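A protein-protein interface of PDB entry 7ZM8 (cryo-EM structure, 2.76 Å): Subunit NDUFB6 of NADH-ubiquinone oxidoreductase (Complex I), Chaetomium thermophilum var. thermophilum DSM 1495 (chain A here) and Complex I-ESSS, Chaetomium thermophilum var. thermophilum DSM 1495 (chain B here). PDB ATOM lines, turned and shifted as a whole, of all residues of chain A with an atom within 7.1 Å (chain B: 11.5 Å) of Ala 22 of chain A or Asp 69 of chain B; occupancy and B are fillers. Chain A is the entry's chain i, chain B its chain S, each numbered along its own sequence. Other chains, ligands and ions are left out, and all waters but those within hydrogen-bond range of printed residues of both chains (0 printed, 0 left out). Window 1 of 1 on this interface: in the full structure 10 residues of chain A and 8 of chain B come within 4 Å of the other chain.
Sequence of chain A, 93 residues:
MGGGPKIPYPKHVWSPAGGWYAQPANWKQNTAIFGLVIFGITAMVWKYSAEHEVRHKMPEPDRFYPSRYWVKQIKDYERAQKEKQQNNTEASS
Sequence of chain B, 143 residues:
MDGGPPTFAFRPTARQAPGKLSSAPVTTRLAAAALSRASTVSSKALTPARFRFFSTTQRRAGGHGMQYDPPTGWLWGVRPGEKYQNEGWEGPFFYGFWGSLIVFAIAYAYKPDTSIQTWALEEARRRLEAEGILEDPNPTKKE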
ATOM      1  N   LYS A   6      11.975  23.776   0.407  1.00  0.00           N
ATOM      2  CA  LYS A   6      10.836  24.094  -0.438  1.00  0.00           C
ATOM      3  C   LYS A   6       9.627  24.407   0.432  1.00  0.00           C
ATOM      4  O   LYS A   6       9.454  23.827   1.506  1.00  0.00           O
ATOM      5  CB  LYS A   6      10.532  22.945  -1.402  1.00  0.00           C
ATOM      6  CG  LYS A   6      11.525  22.859  -2.551  1.00  0.00           C
ATOM      7  CD  LYS A   6      10.987  22.092  -3.740  1.00  0.00           C
ATOM      8  CE  LYS A   6      10.754  20.638  -3.411  1.00  0.00           C
ATOM      9  NZ  LYS A   6      10.279  19.877  -4.590  1.00  0.00           N
ATOM     10  N   ILE A   7       8.816  25.347  -0.030  1.00  0.00           N
ATOM     11  CA  ILE A   7       7.653  25.811   0.735  1.00  0.00           C
ATOM     12  C   ILE A   7       6.626  24.690   0.834  1.00  0.00           C
ATOM     13  O   ILE A   7       6.398  23.974  -0.156  1.00  0.00           O
ATOM     14  CB  ILE A   7       7.050  27.060   0.077  1.00  0.00           C
ATOM     15  CG1 ILE A   7       8.044  28.225   0.087  1.00  0.00           C
ATOM     16  CG2 ILE A   7       5.758  27.469   0.745  1.00  0.00           C
ATOM     17  CD1 ILE A   7       8.958  28.299  -1.097  1.00  0.00           C
ATOM     18  N   TYR A   9       2.943  23.440   0.593  1.00  0.00           N
ATOM     19  CA  TYR A   9       1.830  23.946  -0.192  1.00  0.00           C
ATOM     20  C   TYR A   9       0.714  22.916  -0.212  1.00  0.00           C
ATOM     21  O   TYR A   9       0.953  21.728   0.029  1.00  0.00           O
ATOM     22  CB  TYR A   9       2.267  24.290  -1.622  1.00  0.00           C
ATOM     23  CG  TYR A   9       2.771  23.117  -2.416  1.00  0.00           C
ATOM     24  CD1 TYR A   9       4.074  22.679  -2.281  1.00  0.00           C
ATOM     25  CD2 TYR A   9       1.946  22.453  -3.305  1.00  0.00           C
ATOM     26  CE1 TYR A   9       4.537  21.613  -3.002  1.00  0.00           C
ATOM     27  CE2 TYR A   9       2.399  21.384  -4.030  1.00  0.00           C
ATOM     28  CZ  TYR A   9       3.694  20.969  -3.876  1.00  0.00           C
ATOM     29  OH  TYR A   9       4.159  19.900  -4.595  1.00  0.00           O
ATOM     30  N   LYS A  11      -1.897  20.350  -1.800  1.00  0.00           N
ATOM     31  CA  LYS A  11      -1.767  19.461  -2.942  1.00  0.00           C
ATOM     32  C   LYS A  11      -3.081  19.218  -3.670  1.00  0.00           C
ATOM     33  O   LYS A  11      -3.105  18.465  -4.644  1.00  0.00           O
ATOM     34  CB  LYS A  11      -1.159  18.139  -2.491  1.00  0.00           C
ATOM     35  CG  LYS A  11      -0.029  18.318  -1.503  1.00  0.00           C
ATOM     36  CD  LYS A  11       1.285  18.546  -2.211  1.00  0.00           C
ATOM     37  CE  LYS A  11       2.448  18.491  -1.243  1.00  0.00           C
ATOM     38  NZ  LYS A  11       2.621  19.779  -0.515  1.00  0.00           N
ATOM     39  N   SER A  15      -3.753  24.268 -10.829  1.00  0.00           N
ATOM     40  CA  SER A  15      -3.412  25.494 -11.520  1.00  0.00           C
ATOM     41  C   SER A  15      -3.008  25.179 -12.951  1.00  0.00           C
ATOM     42  O   SER A  15      -2.295  24.204 -13.185  1.00  0.00           O
ATOM     43  CB  SER A  15      -2.268  26.220 -10.808  1.00  0.00           C
ATOM     44  OG  SER A  15      -1.624  27.118 -11.685  1.00  0.00           O
ATOM     45  N   ALA A  17      -0.861  26.731 -14.688  1.00  0.00           N
ATOM     46  CA  ALA A  17       0.560  27.006 -14.816  1.00  0.00           C
ATOM     47  C   ALA A  17       1.417  26.036 -14.021  1.00  0.00           C
ATOM     48  O   ALA A  17       2.635  26.192 -13.985  1.00  0.00           O
ATOM     49  CB  ALA A  17       0.858  28.440 -14.387  1.00  0.00           C
ATOM     50  N   GLY A  18       0.802  25.040 -13.384  1.00  0.00           N
ATOM     51  CA  GLY A  18       1.500  23.982 -12.693  1.00  0.00           C
ATOM     52  C   GLY A  18       1.378  24.048 -11.186  1.00  0.00           C
ATOM     53  O   GLY A  18       1.153  23.015 -10.548  1.00  0.00           O
ATOM     54  N   GLY A  19       1.495  25.228 -10.607  1.00  0.00           N
ATOM     55  CA  GLY A  19       1.462  25.374  -9.163  1.00  0.00           C
ATOM     56  C   GLY A  19       2.848  25.654  -8.596  1.00  0.00           C
ATOM     57  O   GLY A  19       3.549  26.539  -9.071  1.00  0.00           O
ATOM     58  N   TRP A  20       3.242  24.879  -7.587  1.00  0.00           N
ATOM     59  CA  TRP A  20       4.430  25.214  -6.810  1.00  0.00           C
ATOM     60  C   TRP A  20       5.734  24.636  -7.346  1.00  0.00           C
ATOM     61  O   TRP A  20       6.716  25.365  -7.454  1.00  0.00           O
ATOM     62  CB  TRP A  20       4.222  24.836  -5.346  1.00  0.00           C
ATOM     63  CG  TRP A  20       3.345  25.813  -4.628  1.00  0.00           C
ATOM     64  CD1 TRP A  20       3.766  26.883  -3.916  1.00  0.00           C
ATOM     65  CD2 TRP A  20       1.917  25.888  -4.652  1.00  0.00           C
ATOM     66  NE1 TRP A  20       2.699  27.584  -3.431  1.00  0.00           N
ATOM     67  CE2 TRP A  20       1.549  26.997  -3.878  1.00  0.00           C
ATOM     68  CE3 TRP A  20       0.913  25.106  -5.222  1.00  0.00           C
ATOM     69  CZ2 TRP A  20       0.225  27.346  -3.659  1.00  0.00           C
ATOM     70  CZ3 TRP A  20      -0.399  25.458  -5.005  1.00  0.00           C
ATOM     71  CH2 TRP A  20      -0.731  26.566  -4.231  1.00  0.00           C
ATOM     72  N   TYR A  21       5.827  23.371  -7.703  1.00  0.00           N
ATOM     73  CA  TYR A  21       7.137  22.922  -8.255  1.00  0.00           C
ATOM     74  C   TYR A  21       6.789  21.900  -9.312  1.00  0.00           C
ATOM     75  O   TYR A  21       7.396  20.830  -9.313  1.00  0.00           O
ATOM     76  CB  TYR A  21       8.053  22.360  -7.168  1.00  0.00           C
ATOM     77  CG  TYR A  21       8.503  23.359  -6.133  1.00  0.00           C
ATOM     78  CD1 TYR A  21       9.567  24.209  -6.382  1.00  0.00           C
ATOM     79  CD2 TYR A  21       7.854  23.469  -4.914  1.00  0.00           C
ATOM     80  CE1 TYR A  21       9.981  25.138  -5.444  1.00  0.00           C
ATOM     81  CE2 TYR A  21       8.251  24.397  -3.967  1.00  0.00           C
ATOM     82  CZ  TYR A  21       9.322  25.229  -4.233  1.00  0.00           C
ATOM     83  OH  TYR A  21       9.737  26.139  -3.308  1.00  0.00           O
ATOM     84  N   ALA A  22       5.902  22.253 -10.231  1.00  0.00           N
ATOM     85  CA  ALA A  22       5.371  21.189 -11.097  1.00  0.00           C
ATOM     86  C   ALA A  22       6.178  20.905 -12.353  1.00  0.00           C
ATOM     87  O   ALA A  22       6.258  21.782 -13.226  1.00  0.00           O
ATOM     88  CB  ALA A  22       3.927  21.470 -11.403  1.00  0.00           C
ATOM     89  N   GLN A  23       6.762  19.714 -12.408  1.00  0.00           N
ATOM     90  CA  GLN A  23       7.413  19.261 -13.651  1.00  0.00           C
ATOM     91  C   GLN A  23       6.890  17.846 -13.845  1.00  0.00           C
ATOM     92  O   GLN A  23       7.104  17.030 -12.947  1.00  0.00           O
ATOM     93  CB  GLN A  23       8.929  19.293 -13.518  1.00  0.00           C
ATOM     94  CG  GLN A  23       9.662  18.627 -14.667  1.00  0.00           C
ATOM     95  CD  GLN A  23      10.888  19.433 -15.005  1.00  0.00           C
ATOM     96  OE1 GLN A  23      10.839  20.658 -15.059  1.00  0.00           O
ATOM     97  NE2 GLN A  23      11.999  18.749 -15.220  1.00  0.00           N
ATOM     98  N   PRO A  24       6.186  17.523 -14.943  1.00  0.00           N
ATOM     99  CA  PRO A  24       5.761  16.151 -15.173  1.00  0.00           C
ATOM    100  C   PRO A  24       6.945  15.274 -15.602  1.00  0.00           C
ATOM    101  O   PRO A  24       7.969  15.815 -15.947  1.00  0.00           O
ATOM    102  CB  PRO A  24       4.678  16.302 -16.247  1.00  0.00           C
ATOM    103  CG  PRO A  24       5.033  17.575 -16.975  1.00  0.00           C
ATOM    104  CD  PRO A  24       5.702  18.461 -15.950  1.00  0.00           C
ATOM    105  N   TRP A  27       7.382  15.580 -19.269  1.00  0.00           N
ATOM    106  CA  TRP A  27       7.609  16.999 -19.646  1.00  0.00           C
ATOM    107  C   TRP A  27       8.246  17.105 -21.031  1.00  0.00           C
ATOM    108  O   TRP A  27       7.804  17.967 -21.800  1.00  0.00           O
ATOM    109  CB  TRP A  27       8.381  17.753 -18.557  1.00  0.00           C
ATOM    110  CG  TRP A  27       9.872  17.607 -18.531  1.00  0.00           C
ATOM    111  CD1 TRP A  27      10.606  16.801 -17.712  1.00  0.00           C
ATOM    112  CD2 TRP A  27      10.822  18.346 -19.318  1.00  0.00           C
ATOM    113  NE1 TRP A  27      11.942  16.966 -17.953  1.00  0.00           N
ATOM    114  CE2 TRP A  27      12.105  17.907 -18.934  1.00  0.00           C
ATOM    115  CE3 TRP A  27      10.716  19.317 -20.319  1.00  0.00           C
ATOM    116  CZ2 TRP A  27      13.267  18.410 -19.516  1.00  0.00           C
ATOM    117  CZ3 TRP A  27      11.863  19.805 -20.901  1.00  0.00           C
ATOM    118  CH2 TRP A  27      13.121  19.356 -20.502  1.00  0.00           C
ATOM    119  N   GLN B  67      14.805  19.248  -8.058  1.00  0.00           N
ATOM    120  CA  GLN B  67      13.939  18.238  -7.465  1.00  0.00           C
ATOM    121  C   GLN B  67      12.490  18.660  -7.579  1.00  0.00           C
ATOM    122  O   GLN B  67      11.826  18.924  -6.585  1.00  0.00           O
ATOM    123  CB  GLN B  67      14.308  17.999  -6.002  1.00  0.00           C
ATOM    124  CG  GLN B  67      15.637  17.290  -5.815  1.00  0.00           C
ATOM    125  CD  GLN B  67      15.730  16.017  -6.631  1.00  0.00           C
ATOM    126  OE1 GLN B  67      15.084  15.018  -6.320  1.00  0.00           O
ATOM    127  NE2 GLN B  67      16.536  16.049  -7.686  1.00  0.00           N
ATOM    128  N   TYR B  68      12.022  18.765  -8.818  1.00  0.00           N
ATOM    129  CA  TYR B  68      10.650  19.273  -9.038  1.00  0.00           C
ATOM    130  C   TYR B  68       9.620  18.262  -8.529  1.00  0.00           C
ATOM    131  O   TYR B  68       9.826  17.045  -8.670  1.00  0.00           O
ATOM    132  CB  TYR B  68      10.493  19.686 -10.501  1.00  0.00           C
ATOM    133  CG  TYR B  68      11.412  20.802 -10.924  1.00  0.00           C
ATOM    134  CD1 TYR B  68      11.394  22.025 -10.275  1.00  0.00           C
ATOM    135  CD2 TYR B  68      12.298  20.639 -11.974  1.00  0.00           C
ATOM    136  CE1 TYR B  68      12.236  23.056 -10.656  1.00  0.00           C
ATOM    137  CE2 TYR B  68      13.142  21.661 -12.372  1.00  0.00           C
ATOM    138  CZ  TYR B  68      13.113  22.872 -11.709  1.00  0.00           C
ATOM    139  OH  TYR B  68      13.945  23.883 -12.094  1.00  0.00           O
ATOM    140  N   ASP B  69       8.532  18.768  -7.959  1.00  0.00           N
ATOM    141  CA  ASP B  69       7.474  17.910  -7.381  1.00  0.00           C
ATOM    142  C   ASP B  69       6.572  17.367  -8.488  1.00  0.00           C
ATOM    143  O   ASP B  69       6.599  17.921  -9.597  1.00  0.00           O
ATOM    144  CB  ASP B  69       6.678  18.715  -6.357  1.00  0.00           C
ATOM    145  CG  ASP B  69       7.372  18.828  -5.014  1.00  0.00           C
ATOM    146  OD1 ASP B  69       8.104  17.884  -4.657  1.00  0.00           O
ATOM    147  OD2 ASP B  69       7.187  19.860  -4.343  1.00  0.00           O
ATOM    148  N   PRO B  70       5.786  16.295  -8.244  1.00  0.00           N
ATOM    149  CA  PRO B  70       4.831  15.815  -9.229  1.00  0.00           C
ATOM    150  C   PRO B  70       3.747  16.869  -9.477  1.00  0.00           C
ATOM    151  O   PRO B  70       3.514  17.681  -8.600  1.00  0.00           O
ATOM    152  CB  PRO B  70       4.171  14.631  -8.522  1.00  0.00           C
ATOM    153  CG  PRO B  70       4.465  14.825  -7.060  1.00  0.00           C
ATOM    154  CD  PRO B  70       5.834  15.461  -7.046  1.00  0.00           C
ATOM    155  N   PRO B  71       3.064  16.891 -10.644  1.00  0.00           N
ATOM    156  CA  PRO B  71       1.997  17.860 -10.837  1.00  0.00           C
ATOM    157  C   PRO B  71       0.826  17.385  -9.977  1.00  0.00           C
ATOM    158  O   PRO B  71       0.699  16.196  -9.783  1.00  0.00           O
ATOM    159  CB  PRO B  71       1.685  17.764 -12.332  1.00  0.00           C
ATOM    160  CG  PRO B  71       2.862  17.019 -12.927  1.00  0.00           C
ATOM    161  CD  PRO B  71       3.338  16.091 -11.832  1.00  0.00           C
ATOM    162  N   THR B  72       0.003  18.311  -9.483  1.00  0.00           N
ATOM    163  CA  THR B  72      -1.017  17.896  -8.490  1.00  0.00           C
ATOM    164  C   THR B  72      -2.343  18.579  -8.762  1.00  0.00           C
ATOM    165  O   THR B  72      -2.523  19.044  -9.874  1.00  0.00           O
ATOM    166  CB  THR B  72      -0.498  18.216  -7.072  1.00  0.00           C
ATOM    167  OG1 THR B  72      -1.146  17.408  -6.091  1.00  0.00           O
ATOM    168  CG2 THR B  72      -0.529  19.683  -6.703  1.00  0.00           C
ATOM    169  N   GLY B  73      -3.250  18.570  -7.785  1.00  0.00           N
ATOM    170  CA  GLY B  73      -4.462  19.355  -7.851  1.00  0.00           C
ATOM    171  C   GLY B  73      -5.665  18.515  -8.234  1.00  0.00           C
ATOM    172  O   GLY B  73      -5.552  17.409  -8.764  1.00  0.00           O
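The backbone carbonyl oxygen (O) of Gln 67 of chain B is in hydrogen-bond range of the side-chain amino group (NZ) of Lys 6 of chain A (2.7 Å). The side-chain amino group (NZ) of Lys 6 of chain A is in salt-bridge range of the side-chain carboxylate (OD1) of Asp 69 of chain B, at 3.0 Å. OH of Tyr 9 of chain A sits at hydrogen-bond distance from OD2 of Asp 69 of chain B (3.0 Å). The backbone NH of Asp 69 of chain B sits at hydrogen-bond distance from the backbone carbonyl oxygen of Tyr 21 of chain A (2.7 Å). O of Asp 69 of chain B lies within hydrogen-bond range of N of Gln 23 of chain A, 3.3 Å away. The side-chain hydroxyl (OG1) of Thr 72 of chain B lies within hydrogen-bond range of the backbone carbonyl oxygen (O) of Lys 11 of chain A, at 2.7 Å. N of Gly 73 of chain B is in hydrogen-bond range of O of Lys 11 of chain A (3.1 Å).
OH of Tyr 21 of chain A lies close to N of Ile 7 of chain A (3.5 Å). The backbone carbonyl oxygen (O) of Tyr 9 of chain A lies within hydrogen-bond range of the side-chain amino group (NZ) of Lys 11 of chain A (2.6 Å). The side-chain amide nitrogen of Gln 23 of chain A sits close to the indole nitrogen of Trp 27 of chain A.
Among the printed residues, merely in contact across the chains: Gln 23 of chain A with Tyr 68 of chain B, Tyr 21 of chain A with Tyr 68 of chain B, Pro 24 of chain A with Pro 71 of chain B and Ala 22 of chain A with Asp 69 of chain B.
Of the printed residues of chain B, Lys 11 of chain A touches Thr 72 (2.7 Å) and Gly 73 (3.1 Å). Ser 15 of chain A touches none of the printed residues of chain B. No residue of chain B comes within 4 Å of Gly 18 of chain A. No residue of chain B comes within 4 Å of Gly 19 of chain A. Of the printed residues of chain B, Tyr 21 of chain A touches Tyr 68 and Asp 69. Of chain B, only Asp 69 comes within 4 Å of Ala 22 of chain A. Gln 23 of chain A touches just these residues of chain B: Tyr 68 and Asp 69. Pro 24 of chain A touches one residue of chain B. Printed residues of chain A within 4 Å of Tyr 68 of chain B: Tyr 21 (3.5 Å) and Gln 23 (3.4 Å). Printed residues of chain A within 4 Å of Pro 71 of chain B: Pro 24. Printed residues of chain A within 4 Å of Thr 72 of chain B: Lys 11 (2.7 Å). Of the printed residues of chain A, Gly 73 of chain B touches Lys 11. The nearest residue of chain A that does not touch Asp 69 of chain B is Pro 24 of chain A (5.4 Å). The nearest printed residue of chain B that does not touch Lys 11 of chain A is Asp 69 of chain B (5.8 Å).
Hydrophobic or aromatic side chains of chain A that line the printed part of chain B: Tyr 9, Tyr 21 and Pro 24. Of the 7 printed residues of chain B, 6 touch a printed residue of chain A. Printed residues of chain B that touch a printed residue of chain A: Gln 67, Tyr 68, Asp 69, Pro 71, Thr 72 and Gly 73. Along chain B the printed residues that touch a printed residue of chain A span positions 67 to 73. Among the printed residues, 11 pairs touch across the chains.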
